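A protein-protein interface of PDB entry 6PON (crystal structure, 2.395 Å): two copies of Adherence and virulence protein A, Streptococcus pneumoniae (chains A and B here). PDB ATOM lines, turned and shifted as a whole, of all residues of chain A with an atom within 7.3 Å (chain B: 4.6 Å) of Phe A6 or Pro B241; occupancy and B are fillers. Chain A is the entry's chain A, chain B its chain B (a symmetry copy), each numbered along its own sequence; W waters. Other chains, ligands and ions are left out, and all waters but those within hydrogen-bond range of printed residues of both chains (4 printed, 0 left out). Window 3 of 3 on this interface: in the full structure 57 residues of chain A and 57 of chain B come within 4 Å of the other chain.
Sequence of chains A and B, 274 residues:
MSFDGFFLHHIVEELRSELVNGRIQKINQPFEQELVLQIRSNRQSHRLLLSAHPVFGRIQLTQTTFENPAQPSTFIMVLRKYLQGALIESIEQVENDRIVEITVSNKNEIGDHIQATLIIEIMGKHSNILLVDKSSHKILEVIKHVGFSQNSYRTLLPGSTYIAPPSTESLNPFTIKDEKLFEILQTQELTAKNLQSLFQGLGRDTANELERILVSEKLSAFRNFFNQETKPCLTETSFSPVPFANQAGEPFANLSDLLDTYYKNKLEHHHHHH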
ATOM      1  N   SER A   2      13.507 -18.689  19.305  1.00  0.00           N
ATOM      2  CA  SER A   2      14.431 -18.140  20.289  1.00  0.00           C
ATOM      3  C   SER A   2      13.743 -17.000  21.069  1.00  0.00           C
ATOM      4  O   SER A   2      13.273 -17.193  22.184  1.00  0.00           O
ATOM      5  N   PHE A   3      13.660 -15.790  20.518  1.00  0.00           N
ATOM      6  CA  PHE A   3      12.748 -14.819  21.118  1.00  0.00           C
ATOM      7  C   PHE A   3      11.320 -15.111  20.638  1.00  0.00           C
ATOM      8  O   PHE A   3      10.693 -14.329  19.923  1.00  0.00           O
ATOM      9  CB  PHE A   3      13.147 -13.377  20.823  1.00  0.00           C
ATOM     10  CG  PHE A   3      12.603 -12.415  21.840  1.00  0.00           C
ATOM     11  CD1 PHE A   3      11.326 -11.904  21.716  1.00  0.00           C
ATOM     12  CD2 PHE A   3      13.337 -12.101  22.982  1.00  0.00           C
ATOM     13  CE1 PHE A   3      10.801 -11.036  22.703  1.00  0.00           C
ATOM     14  CE2 PHE A   3      12.822 -11.257  23.967  1.00  0.00           C
ATOM     15  CZ  PHE A   3      11.553 -10.715  23.824  1.00  0.00           C
ATOM     16  N   ASP A   4      10.796 -16.267  21.071  1.00  0.00           N
ATOM     17  CA  ASP A   4       9.437 -16.678  20.756  1.00  0.00           C
ATOM     18  C   ASP A   4       8.511 -16.325  21.914  1.00  0.00           C
ATOM     19  O   ASP A   4       8.930 -15.788  22.939  1.00  0.00           O
ATOM     20  CB  ASP A   4       9.383 -18.179  20.414  1.00  0.00           C
ATOM     21  CG  ASP A   4       9.798 -19.075  21.567  1.00  0.00           C
ATOM     22  OD1 ASP A   4      10.239 -18.586  22.637  1.00  0.00           O
ATOM     23  OD2 ASP A   4       9.688 -20.306  21.396  1.00  0.00           O
ATOM     24  N   GLY A   5       7.232 -16.641  21.749  1.00  0.00           N
ATOM     25  CA  GLY A   5       6.274 -16.340  22.802  1.00  0.00           C
ATOM     26  C   GLY A   5       6.590 -17.074  24.089  1.00  0.00           C
ATOM     27  O   GLY A   5       6.394 -16.537  25.188  1.00  0.00           O
ATOM     28  N   PHE A   6       7.096 -18.313  23.964  1.00  0.00           N
ATOM     29  CA  PHE A   6       7.534 -19.087  25.118  1.00  0.00           C
ATOM     30  C   PHE A   6       8.579 -18.330  25.926  1.00  0.00           C
ATOM     31  O   PHE A   6       8.461 -18.196  27.148  1.00  0.00           O
ATOM     32  CB  PHE A   6       8.096 -20.430  24.650  1.00  0.00           C
ATOM     33  CG  PHE A   6       8.546 -21.323  25.765  1.00  0.00           C
ATOM     34  CD1 PHE A   6       7.630 -21.841  26.675  1.00  0.00           C
ATOM     35  CD2 PHE A   6       9.880 -21.658  25.910  1.00  0.00           C
ATOM     36  CE1 PHE A   6       8.036 -22.665  27.704  1.00  0.00           C
ATOM     37  CE2 PHE A   6      10.287 -22.511  26.949  1.00  0.00           C
ATOM     38  CZ  PHE A   6       9.354 -23.003  27.847  1.00  0.00           C
ATOM     39  N   PHE A   7       9.617 -17.827  25.253  1.00  0.00           N
ATOM     40  CA  PHE A   7      10.656 -17.059  25.930  1.00  0.00           C
ATOM     41  C   PHE A   7      10.086 -15.768  26.514  1.00  0.00           C
ATOM     42  O   PHE A   7      10.356 -15.405  27.666  1.00  0.00           O
ATOM     43  CB  PHE A   7      11.777 -16.768  24.925  1.00  0.00           C
ATOM     44  CG  PHE A   7      12.961 -16.047  25.503  1.00  0.00           C
ATOM     45  CD1 PHE A   7      14.048 -16.759  25.999  1.00  0.00           C
ATOM     46  CD2 PHE A   7      13.010 -14.644  25.520  1.00  0.00           C
ATOM     47  CE1 PHE A   7      15.141 -16.099  26.524  1.00  0.00           C
ATOM     48  CE2 PHE A   7      14.117 -13.972  26.055  1.00  0.00           C
ATOM     49  CZ  PHE A   7      15.174 -14.700  26.561  1.00  0.00           C
ATOM     50  N   LEU A   8       9.285 -15.058  25.723  1.00  0.00           N
ATOM     51  CA  LEU A   8       8.736 -13.791  26.182  1.00  0.00           C
ATOM     52  C   LEU A   8       7.909 -13.985  27.448  1.00  0.00           C
ATOM     53  O   LEU A   8       7.904 -13.115  28.330  1.00  0.00           O
ATOM     54  CB  LEU A   8       7.891 -13.156  25.076  1.00  0.00           C
ATOM     55  CG  LEU A   8       7.219 -11.840  25.430  1.00  0.00           C
ATOM     56  CD1 LEU A   8       8.284 -10.842  25.843  1.00  0.00           C
ATOM     57  CD2 LEU A   8       6.446 -11.327  24.252  1.00  0.00           C
ATOM     58  N   HIS A   9       7.194 -15.118  27.554  1.00  0.00           N
ATOM     59  CA  HIS A   9       6.448 -15.400  28.776  1.00  0.00           C
ATOM     60  C   HIS A   9       7.361 -15.299  29.994  1.00  0.00           C
ATOM     61  O   HIS A   9       7.031 -14.649  30.989  1.00  0.00           O
ATOM     62  CB  HIS A   9       5.807 -16.787  28.675  1.00  0.00           C
ATOM     63  CG  HIS A   9       5.019 -17.179  29.880  1.00  0.00           C
ATOM     64  ND1 HIS A   9       3.641 -17.170  29.900  1.00  0.00           N
ATOM     65  CD2 HIS A   9       5.410 -17.588  31.109  1.00  0.00           C
ATOM     66  CE1 HIS A   9       3.214 -17.549  31.089  1.00  0.00           C
ATOM     67  NE2 HIS A   9       4.267 -17.822  31.839  1.00  0.00           N
ATOM     68  N   HIS A  10       8.547 -15.905  29.908  1.00  0.00           N
ATOM     69  CA  HIS A  10       9.475 -15.854  31.028  1.00  0.00           C
ATOM     70  C   HIS A  10      10.012 -14.438  31.240  1.00  0.00           C
ATOM     71  O   HIS A  10      10.191 -14.003  32.382  1.00  0.00           O
ATOM     72  CB  HIS A  10      10.603 -16.872  30.807  1.00  0.00           C
ATOM     73  CG  HIS A  10      10.172 -18.294  31.000  1.00  0.00           C
ATOM     74  ND1 HIS A  10      10.409 -18.992  32.165  1.00  0.00           N
ATOM     75  CD2 HIS A  10       9.492 -19.141  30.189  1.00  0.00           C
ATOM     76  CE1 HIS A  10       9.904 -20.209  32.062  1.00  0.00           C
ATOM     77  NE2 HIS A  10       9.343 -20.325  30.871  1.00  0.00           N
ATOM     78  N   ILE A  11      10.267 -13.711  30.149  1.00  0.00           N
ATOM     79  CA  ILE A  11      10.674 -12.303  30.220  1.00  0.00           C
ATOM     80  C   ILE A  11       9.643 -11.483  30.990  1.00  0.00           C
ATOM     81  O   ILE A  11       9.983 -10.704  31.890  1.00  0.00           O
ATOM     82  CB  ILE A  11      10.872 -11.736  28.798  1.00  0.00           C
ATOM     83  CG1 ILE A  11      12.218 -12.145  28.230  1.00  0.00           C
ATOM     84  CG2 ILE A  11      10.742 -10.248  28.786  1.00  0.00           C
ATOM     85  CD1 ILE A  11      13.371 -11.289  28.746  1.00  0.00           C
ATOM     86  N   GLN A  93       1.528  -9.898  28.626  1.00  0.00           N
ATOM     87  CA  GLN A  93       1.655 -10.458  27.303  1.00  0.00           C
ATOM     88  C   GLN A  93       0.253 -10.676  26.752  1.00  0.00           C
ATOM     89  O   GLN A  93      -0.661 -11.030  27.491  1.00  0.00           O
ATOM     90  CB  GLN A  93       2.434 -11.777  27.381  1.00  0.00           C
ATOM     91  CG  GLN A  93       2.717 -12.468  26.054  1.00  0.00           C
ATOM     92  CD  GLN A  93       3.554 -13.739  26.218  1.00  0.00           C
ATOM     93  OE1 GLN A  93       3.835 -14.181  27.344  1.00  0.00           O
ATOM     94  NE2 GLN A  93       3.972 -14.322  25.089  1.00  0.00           N
ATOM     95  N   ASN A  96      -0.023 -15.945  24.264  1.00  0.00           N
ATOM     96  CA  ASN A  96       1.371 -16.320  24.073  1.00  0.00           C
ATOM     97  C   ASN A  96       1.914 -15.778  22.753  1.00  0.00           C
ATOM     98  O   ASN A  96       2.836 -16.351  22.173  1.00  0.00           O
ATOM     99  CB  ASN A  96       1.546 -17.840  24.144  1.00  0.00           C
ATOM    100  CG  ASN A  96       2.968 -18.247  24.500  1.00  0.00           C
ATOM    101  OD1 ASN A  96       3.595 -17.624  25.360  1.00  0.00           O
ATOM    102  ND2 ASN A  96       3.495 -19.282  23.827  1.00  0.00           N
ATOM    103  N   ASP A  97       1.318 -14.697  22.245  1.00  0.00           N
ATOM    104  CA  ASP A  97       1.864 -13.964  21.111  1.00  0.00           C
ATOM    105  C   ASP A  97       3.017 -13.073  21.583  1.00  0.00           C
ATOM    106  O   ASP A  97       3.268 -12.915  22.784  1.00  0.00           O
ATOM    107  CB  ASP A  97       0.770 -13.129  20.423  1.00  0.00           C
ATOM    108  CG  ASP A  97       1.025 -12.933  18.913  1.00  0.00           C
ATOM    109  OD1 ASP A  97       2.099 -13.337  18.420  1.00  0.00           O
ATOM    110  OD2 ASP A  97       0.149 -12.368  18.210  1.00  0.00           O
ATOM    111  N   ARG A  98       3.740 -12.505  20.622  1.00  0.00           N
ATOM    112  CA  ARG A  98       4.899 -11.670  20.935  1.00  0.00           C
ATOM    113  C   ARG A  98       4.497 -10.196  21.019  1.00  0.00           C
ATOM    114  O   ARG A  98       4.940  -9.356  20.246  1.00  0.00           O
ATOM    115  CB  ARG A  98       6.003 -11.891  19.905  1.00  0.00           C
ATOM    116  CG  ARG A  98       6.675 -13.271  19.994  1.00  0.00           C
ATOM    117  CD  ARG A  98       7.668 -13.457  18.856  1.00  0.00           C
ATOM    118  NE  ARG A  98       6.966 -13.414  17.580  1.00  0.00           N
ATOM    119  CZ  ARG A  98       7.556 -13.299  16.397  1.00  0.00           C
ATOM    120  NH1 ARG A  98       8.876 -13.216  16.310  1.00  0.00           N
ATOM    121  NH2 ARG A  98       6.817 -13.268  15.292  1.00  0.00           N
ATOM    122  N   PRO A 173      -0.518 -22.432  24.924  1.00  0.00           N
ATOM    123  CA  PRO A 173      -0.134 -23.623  25.700  1.00  0.00           C
ATOM    124  C   PRO A 173      -0.110 -23.393  27.194  1.00  0.00           C
ATOM    125  O   PRO A 173      -0.255 -24.356  27.958  1.00  0.00           O
ATOM    126  CB  PRO A 173       1.275 -23.937  25.176  1.00  0.00           C
ATOM    127  CG  PRO A 173       1.814 -22.605  24.749  1.00  0.00           C
ATOM    128  CD  PRO A 173       0.623 -21.841  24.199  1.00  0.00           C
ATOM    129  N   PHE A 174       0.066 -22.150  27.635  1.00  0.00           N
ATOM    130  CA  PHE A 174       0.176 -21.862  29.056  1.00  0.00           C
ATOM    131  C   PHE A 174      -1.176 -21.962  29.773  1.00  0.00           C
ATOM    132  O   PHE A 174      -1.222 -22.278  30.966  1.00  0.00           O
ATOM    133  CB  PHE A 174       0.794 -20.462  29.256  1.00  0.00           C
ATOM    134  CG  PHE A 174       2.292 -20.393  29.000  1.00  0.00           C
ATOM    135  CD1 PHE A 174       3.194 -20.778  29.980  1.00  0.00           C
ATOM    136  CD2 PHE A 174       2.787 -19.936  27.792  1.00  0.00           C
ATOM    137  CE1 PHE A 174       4.583 -20.712  29.760  1.00  0.00           C
ATOM    138  CE2 PHE A 174       4.162 -19.868  27.558  1.00  0.00           C
ATOM    139  CZ  PHE A 174       5.068 -20.266  28.548  1.00  0.00           C
ATOM    140  N   GLN A 200       0.237 -21.669  20.095  1.00  0.00           N
ATOM    141  CA  GLN A 200       0.690 -20.340  19.733  1.00  0.00           C
ATOM    142  C   GLN A 200       2.022 -20.023  20.401  1.00  0.00           C
ATOM    143  O   GLN A 200       2.245 -20.357  21.569  1.00  0.00           O
ATOM    144  CB  GLN A 200      -0.369 -19.312  20.127  1.00  0.00           C
ATOM    145  CG  GLN A 200       0.154 -17.909  20.249  1.00  0.00           C
ATOM    146  CD  GLN A 200      -0.869 -17.005  20.868  1.00  0.00           C
ATOM    147  OE1 GLN A 200      -1.330 -17.245  21.994  1.00  0.00           O
ATOM    148  NE2 GLN A 200      -1.257 -15.962  20.133  1.00  0.00           N
ATOM    149  N   GLY A 201       2.920 -19.408  19.631  1.00  0.00           N
ATOM    150  CA  GLY A 201       4.104 -18.781  20.186  1.00  0.00           C
ATOM    151  C   GLY A 201       5.246 -19.709  20.518  1.00  0.00           C
ATOM    152  O   GLY A 201       6.010 -19.439  21.446  1.00  0.00           O
ATOM    153  N   LEU A 202       5.387 -20.802  19.797  1.00  0.00           N
ATOM    154  CA  LEU A 202       6.500 -21.719  19.982  1.00  0.00           C
ATOM    155  C   LEU A 202       7.447 -21.578  18.799  1.00  0.00           C
ATOM    156  O   LEU A 202       7.043 -21.809  17.653  1.00  0.00           O
ATOM    157  CB  LEU A 202       6.003 -23.161  20.097  1.00  0.00           C
ATOM    158  CG  LEU A 202       5.051 -23.435  21.259  1.00  0.00           C
ATOM    159  CD1 LEU A 202       4.733 -24.930  21.306  1.00  0.00           C
ATOM    160  CD2 LEU A 202       5.616 -22.946  22.596  1.00  0.00           C
ATOM    161  N   GLY A 203       8.691 -21.200  19.077  1.00  0.00           N
ATOM    162  CA  GLY A 203       9.715 -21.243  18.059  1.00  0.00           C
ATOM    163  C   GLY A 203      10.109 -22.664  17.700  1.00  0.00           C
ATOM    164  O   GLY A 203       9.828 -23.641  18.411  1.00  0.00           O
ATOM    165  N   THR A 206      12.104 -24.175  20.471  1.00  0.00           N
ATOM    166  CA  THR A 206      11.227 -24.516  21.581  1.00  0.00           C
ATOM    167  C   THR A 206      10.414 -25.751  21.245  1.00  0.00           C
ATOM    168  O   THR A 206      10.336 -26.697  22.037  1.00  0.00           O
ATOM    169  CB  THR A 206      10.303 -23.343  21.905  1.00  0.00           C
ATOM    170  OG1 THR A 206      11.081 -22.185  22.247  1.00  0.00           O
ATOM    171  CG2 THR A 206       9.377 -23.705  23.063  1.00  0.00           C
ATOM    172  N   ALA A 207       9.832 -25.769  20.042  1.00  0.00           N
ATOM    173  CA  ALA A 207       9.001 -26.892  19.624  1.00  0.00           C
ATOM    174  C   ALA A 207       9.809 -28.187  19.557  1.00  0.00           C
ATOM    175  O   ALA A 207       9.358 -29.231  20.035  1.00  0.00           O
ATOM    176  CB  ALA A 207       8.350 -26.574  18.272  1.00  0.00           C
ATOM    177  N   GLU A 209      12.376 -28.853  21.336  1.00  0.00           N
ATOM    178  CA  GLU A 209      12.663 -29.268  22.702  1.00  0.00           C
ATOM    179  C   GLU A 209      11.431 -29.862  23.366  1.00  0.00           C
ATOM    180  O   GLU A 209      11.547 -30.826  24.123  1.00  0.00           O
ATOM    181  CB  GLU A 209      13.199 -28.096  23.524  1.00  0.00           C
ATOM    182  CG  GLU A 209      13.356 -28.443  25.004  1.00  0.00           C
ATOM    183  CD  GLU A 209      14.556 -29.328  25.289  1.00  0.00           C
ATOM    184  OE1 GLU A 209      15.267 -29.725  24.335  1.00  0.00           O
ATOM    185  OE2 GLU A 209      14.802 -29.605  26.477  1.00  0.00           O
ATOM    186  N   PHE B 225       6.602 -28.372  31.507  1.00  0.00           N
ATOM    187  CA  PHE B 225       7.416 -27.599  30.584  1.00  0.00           C
ATOM    188  C   PHE B 225       6.956 -26.150  30.532  1.00  0.00           C
ATOM    189  O   PHE B 225       7.784 -25.242  30.410  1.00  0.00           O
ATOM    190  CB  PHE B 225       7.371 -28.255  29.194  1.00  0.00           C
ATOM    191  CG  PHE B 225       8.245 -27.597  28.180  1.00  0.00           C
ATOM    192  CD1 PHE B 225       9.590 -27.900  28.108  1.00  0.00           C
ATOM    193  CD2 PHE B 225       7.727 -26.681  27.287  1.00  0.00           C
ATOM    194  CE1 PHE B 225      10.413 -27.289  27.160  1.00  0.00           C
ATOM    195  CE2 PHE B 225       8.537 -26.077  26.347  1.00  0.00           C
ATOM    196  CZ  PHE B 225       9.884 -26.385  26.278  1.00  0.00           C
ATOM    197  N   PHE B 226       5.652 -25.917  30.663  1.00  0.00           N
ATOM    198  CA  PHE B 226       5.065 -24.582  30.615  1.00  0.00           C
ATOM    199  C   PHE B 226       4.805 -23.998  31.991  1.00  0.00           C
ATOM    200  O   PHE B 226       4.148 -22.955  32.098  1.00  0.00           O
ATOM    201  CB  PHE B 226       3.761 -24.598  29.822  1.00  0.00           C
ATOM    202  CG  PHE B 226       3.973 -24.828  28.366  1.00  0.00           C
ATOM    203  CD1 PHE B 226       4.422 -23.797  27.551  1.00  0.00           C
ATOM    204  CD2 PHE B 226       3.786 -26.076  27.820  1.00  0.00           C
ATOM    205  CE1 PHE B 226       4.645 -23.997  26.234  1.00  0.00           C
ATOM    206  CE2 PHE B 226       3.999 -26.289  26.487  1.00  0.00           C
ATOM    207  CZ  PHE B 226       4.438 -25.252  25.686  1.00  0.00           C
ATOM    208  N   THR B 230      12.345 -20.291  35.594  1.00  0.00           N
ATOM    209  CA  THR B 230      13.217 -19.706  34.576  1.00  0.00           C
ATOM    210  C   THR B 230      14.675 -20.067  34.861  1.00  0.00           C
ATOM    211  O   THR B 230      15.145 -19.950  36.000  1.00  0.00           O
ATOM    212  CB  THR B 230      13.045 -18.169  34.534  1.00  0.00           C
ATOM    213  OG1 THR B 230      11.675 -17.825  34.281  1.00  0.00           O
ATOM    214  CG2 THR B 230      13.893 -17.550  33.437  1.00  0.00           C
ATOM    215  N   LYS B 231      15.385 -20.506  33.822  1.00  0.00           N
ATOM    216  CA  LYS B 231      16.794 -20.889  33.907  1.00  0.00           C
ATOM    217  C   LYS B 231      17.477 -20.441  32.627  1.00  0.00           C
ATOM    218  O   LYS B 231      17.641 -21.225  31.686  1.00  0.00           O
ATOM    219  CB  LYS B 231      16.956 -22.400  34.082  1.00  0.00           C
ATOM    220  CG  LYS B 231      16.352 -22.967  35.345  1.00  0.00           C
ATOM    221  CD  LYS B 231      17.435 -23.326  36.341  1.00  0.00           C
ATOM    222  CE  LYS B 231      16.877 -23.507  37.744  1.00  0.00           C
ATOM    223  NZ  LYS B 231      16.366 -22.223  38.298  1.00  0.00           N
ATOM    224  N   PRO B 232      17.902 -19.181  32.555  1.00  0.00           N
ATOM    225  CA  PRO B 232      18.427 -18.655  31.286  1.00  0.00           C
ATOM    226  C   PRO B 232      19.693 -19.383  30.843  1.00  0.00           C
ATOM    227  O   PRO B 232      20.630 -19.564  31.621  1.00  0.00           O
ATOM    228  CB  PRO B 232      18.702 -17.180  31.605  1.00  0.00           C
ATOM    229  CG  PRO B 232      17.936 -16.892  32.850  1.00  0.00           C
ATOM    230  CD  PRO B 232      17.905 -18.168  33.616  1.00  0.00           C
ATOM    231  N   SER B 240      17.571 -19.736  25.324  1.00  0.00           N
ATOM    232  CA  SER B 240      16.350 -20.347  25.805  1.00  0.00           C
ATOM    233  C   SER B 240      16.106 -19.862  27.220  1.00  0.00           C
ATOM    234  O   SER B 240      17.037 -19.415  27.898  1.00  0.00           O
ATOM    235  CB  SER B 240      16.442 -21.882  25.746  1.00  0.00           C
ATOM    236  OG  SER B 240      17.536 -22.409  26.486  1.00  0.00           O
ATOM    237  N   PRO B 241      14.852 -19.904  27.681  1.00  0.00           N
ATOM    238  CA  PRO B 241      14.529 -19.436  29.036  1.00  0.00           C
ATOM    239  C   PRO B 241      14.627 -20.536  30.068  1.00  0.00           C
ATOM    240  O   PRO B 241      14.544 -20.256  31.269  1.00  0.00           O
ATOM    241  CB  PRO B 241      13.085 -18.977  28.891  1.00  0.00           C
ATOM    242  CG  PRO B 241      12.513 -19.995  27.900  1.00  0.00           C
ATOM    243  CD  PRO B 241      13.647 -20.337  26.947  1.00  0.00           C
ATOM    244  N   VAL B 242      14.709 -21.774  29.600  1.00  0.00           N
ATOM    245  CA  VAL B 242      15.103 -22.943  30.378  1.00  0.00           C
ATOM    246  C   VAL B 242      16.080 -23.718  29.514  1.00  0.00           C
ATOM    247  O   VAL B 242      16.179 -23.476  28.301  1.00  0.00           O
ATOM    248  CB  VAL B 242      13.887 -23.823  30.763  1.00  0.00           C
ATOM    249  CG1 VAL B 242      12.859 -23.029  31.555  1.00  0.00           C
ATOM    250  CG2 VAL B 242      13.231 -24.442  29.533  1.00  0.00           C
ATOM    251  N   PHE B 244      17.734 -26.101  27.010  1.00  0.00           N
ATOM    252  CA  PHE B 244      17.348 -26.947  25.890  1.00  0.00           C
ATOM    253  C   PHE B 244      18.415 -28.020  25.668  1.00  0.00           C
ATOM    254  O   PHE B 244      19.506 -27.972  26.235  1.00  0.00           O
ATOM    255  CB  PHE B 244      17.154 -26.106  24.618  1.00  0.00           C
ATOM    256  CG  PHE B 244      15.903 -25.275  24.604  1.00  0.00           C
ATOM    257  CD1 PHE B 244      15.055 -25.238  25.696  1.00  0.00           C
ATOM    258  CD2 PHE B 244      15.576 -24.528  23.471  1.00  0.00           C
ATOM    259  CE1 PHE B 244      13.902 -24.448  25.677  1.00  0.00           C
ATOM    260  CE2 PHE B 244      14.427 -23.750  23.419  1.00  0.00           C
ATOM    261  CZ  PHE B 244      13.581 -23.692  24.528  1.00  0.00           C
ATOM    262  N   LEU B 255      17.338 -13.237  32.526  1.00  0.00           N
ATOM    263  CA  LEU B 255      17.235 -13.152  31.082  1.00  0.00           C
ATOM    264  C   LEU B 255      17.912 -11.902  30.541  1.00  0.00           C
ATOM    265  O   LEU B 255      18.331 -11.896  29.380  1.00  0.00           O
ATOM    266  CB  LEU B 255      15.760 -13.207  30.681  1.00  0.00           C
ATOM    267  CG  LEU B 255      15.038 -14.425  31.271  1.00  0.00           C
ATOM    268  CD1 LEU B 255      13.538 -14.194  31.451  1.00  0.00           C
ATOM    269  CD2 LEU B 255      15.297 -15.647  30.418  1.00  0.00           C
HETATM  270  O   HOH W   1       0.839 -22.742  32.411  1.00  0.00           O
HETATM  271  O   HOH W   2       7.771 -22.431  31.022  1.00  0.00           O
HETATM  272  O   HOH W   3      17.879 -29.758  28.101  1.00  0.00           O
HETATM  273  O   HOH W   4      11.017 -14.980  34.956  1.00  0.00           O
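The side-chain hydroxyl (OG1) of Thr B230 is in hydrogen-bond range of a ring nitrogen (ND1) of His A10 (2.7 Å).
The side-chain hydroxyl (OG) of Ser B240 lies within hydrogen-bond range of the backbone carbonyl oxygen (O) of Val B242 (2.5 Å).
O of Gly A201 lies within hydrogen-bond range of N of Phe A6 (3.0 Å).
OD1 of Asp A4 is in hydrogen-bond range of N of Phe A7, at 2.8 Å.
O of Pro B241 sits at hydrogen-bond distance from N of Lys B231 (2.7 Å).
OD1 of Asp A4 lies close to N of Phe A6, 3.4 Å away.
OG1 of Thr A206 is in hydrogen-bond range of OD2 of Asp A4 (2.5 Å).
Among the printed residues, merely in contact across the chains: Phe A174 with Phe B226, Pro A173 with Phe B226, His A10 with Leu B255, Phe A6 with Pro B241, Phe A6 with Phe B225, Ile A11 with Leu B255, Phe A7 with Pro B241, His A10 with Pro B241, Glu A209 with Phe B244, Thr A206 with Phe B244, Phe A6 with Phe B226, Glu A209 with Phe B225, Leu A202 with Phe B226, Phe A7 with Ser B240 and Phe A7 with Leu B255.
Of chain B, only Phe B225 (3.5 Å), Phe B226 (3.7 Å) and Pro B241 (3.5 Å) come within 4 Å of Phe A6.
Of chain A, only Phe A6, Phe A7 and His A10 come within 4 Å of Pro B241.
Printed residues of chain A within 4 Å of Leu B255: Phe A7, His A10 and Ile A11.
Printed residues of chain B within 4 Å of His A10: Thr B230, Pro B241 and Leu B255.
The nearest residue of chain A that does not touch Pro B241 is Thr A206 (5.7 Å).
Of the 10 printed residues of chain B, 7 touch a printed residue of chain A.
Hydrophobic or aromatic side chains of chain B within 4 Å of the printed part of chain A: Phe B225, Phe B226, Pro B241, Phe B244 and Leu B255.
Of the 23 printed residues of chain A, 9 touch a printed residue of chain B.
Among the printed residues, 16 pairs touch across the chains.
Among the printed residues, no Asp or Glu carboxylate lies within 4 Å of a Lys or Arg side-chain nitrogen of the other chain.
No position is printed for both chains.
Water W1 bridges O of Phe A174 (2.6 Å) and O of Phe B226 (3.3 Å).
Water W2 lies within hydrogen-bond range of a ring nitrogen (NE2) of His A10 (2.6 Å) and the backbone carbonyl oxygen (O) of Phe B225 (2.9 Å).
Water W4 bridges the backbone carbonyl oxygen (O) of His A10 (2.9 Å) and the side-chain hydroxyl (OG1) of Thr B230 (3.0 Å).
Water W3 bridges the backbone carbonyl oxygen of Phe B244 (3.1 Å) and the side-chain carboxylate of Glu A209 (3.5 Å).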
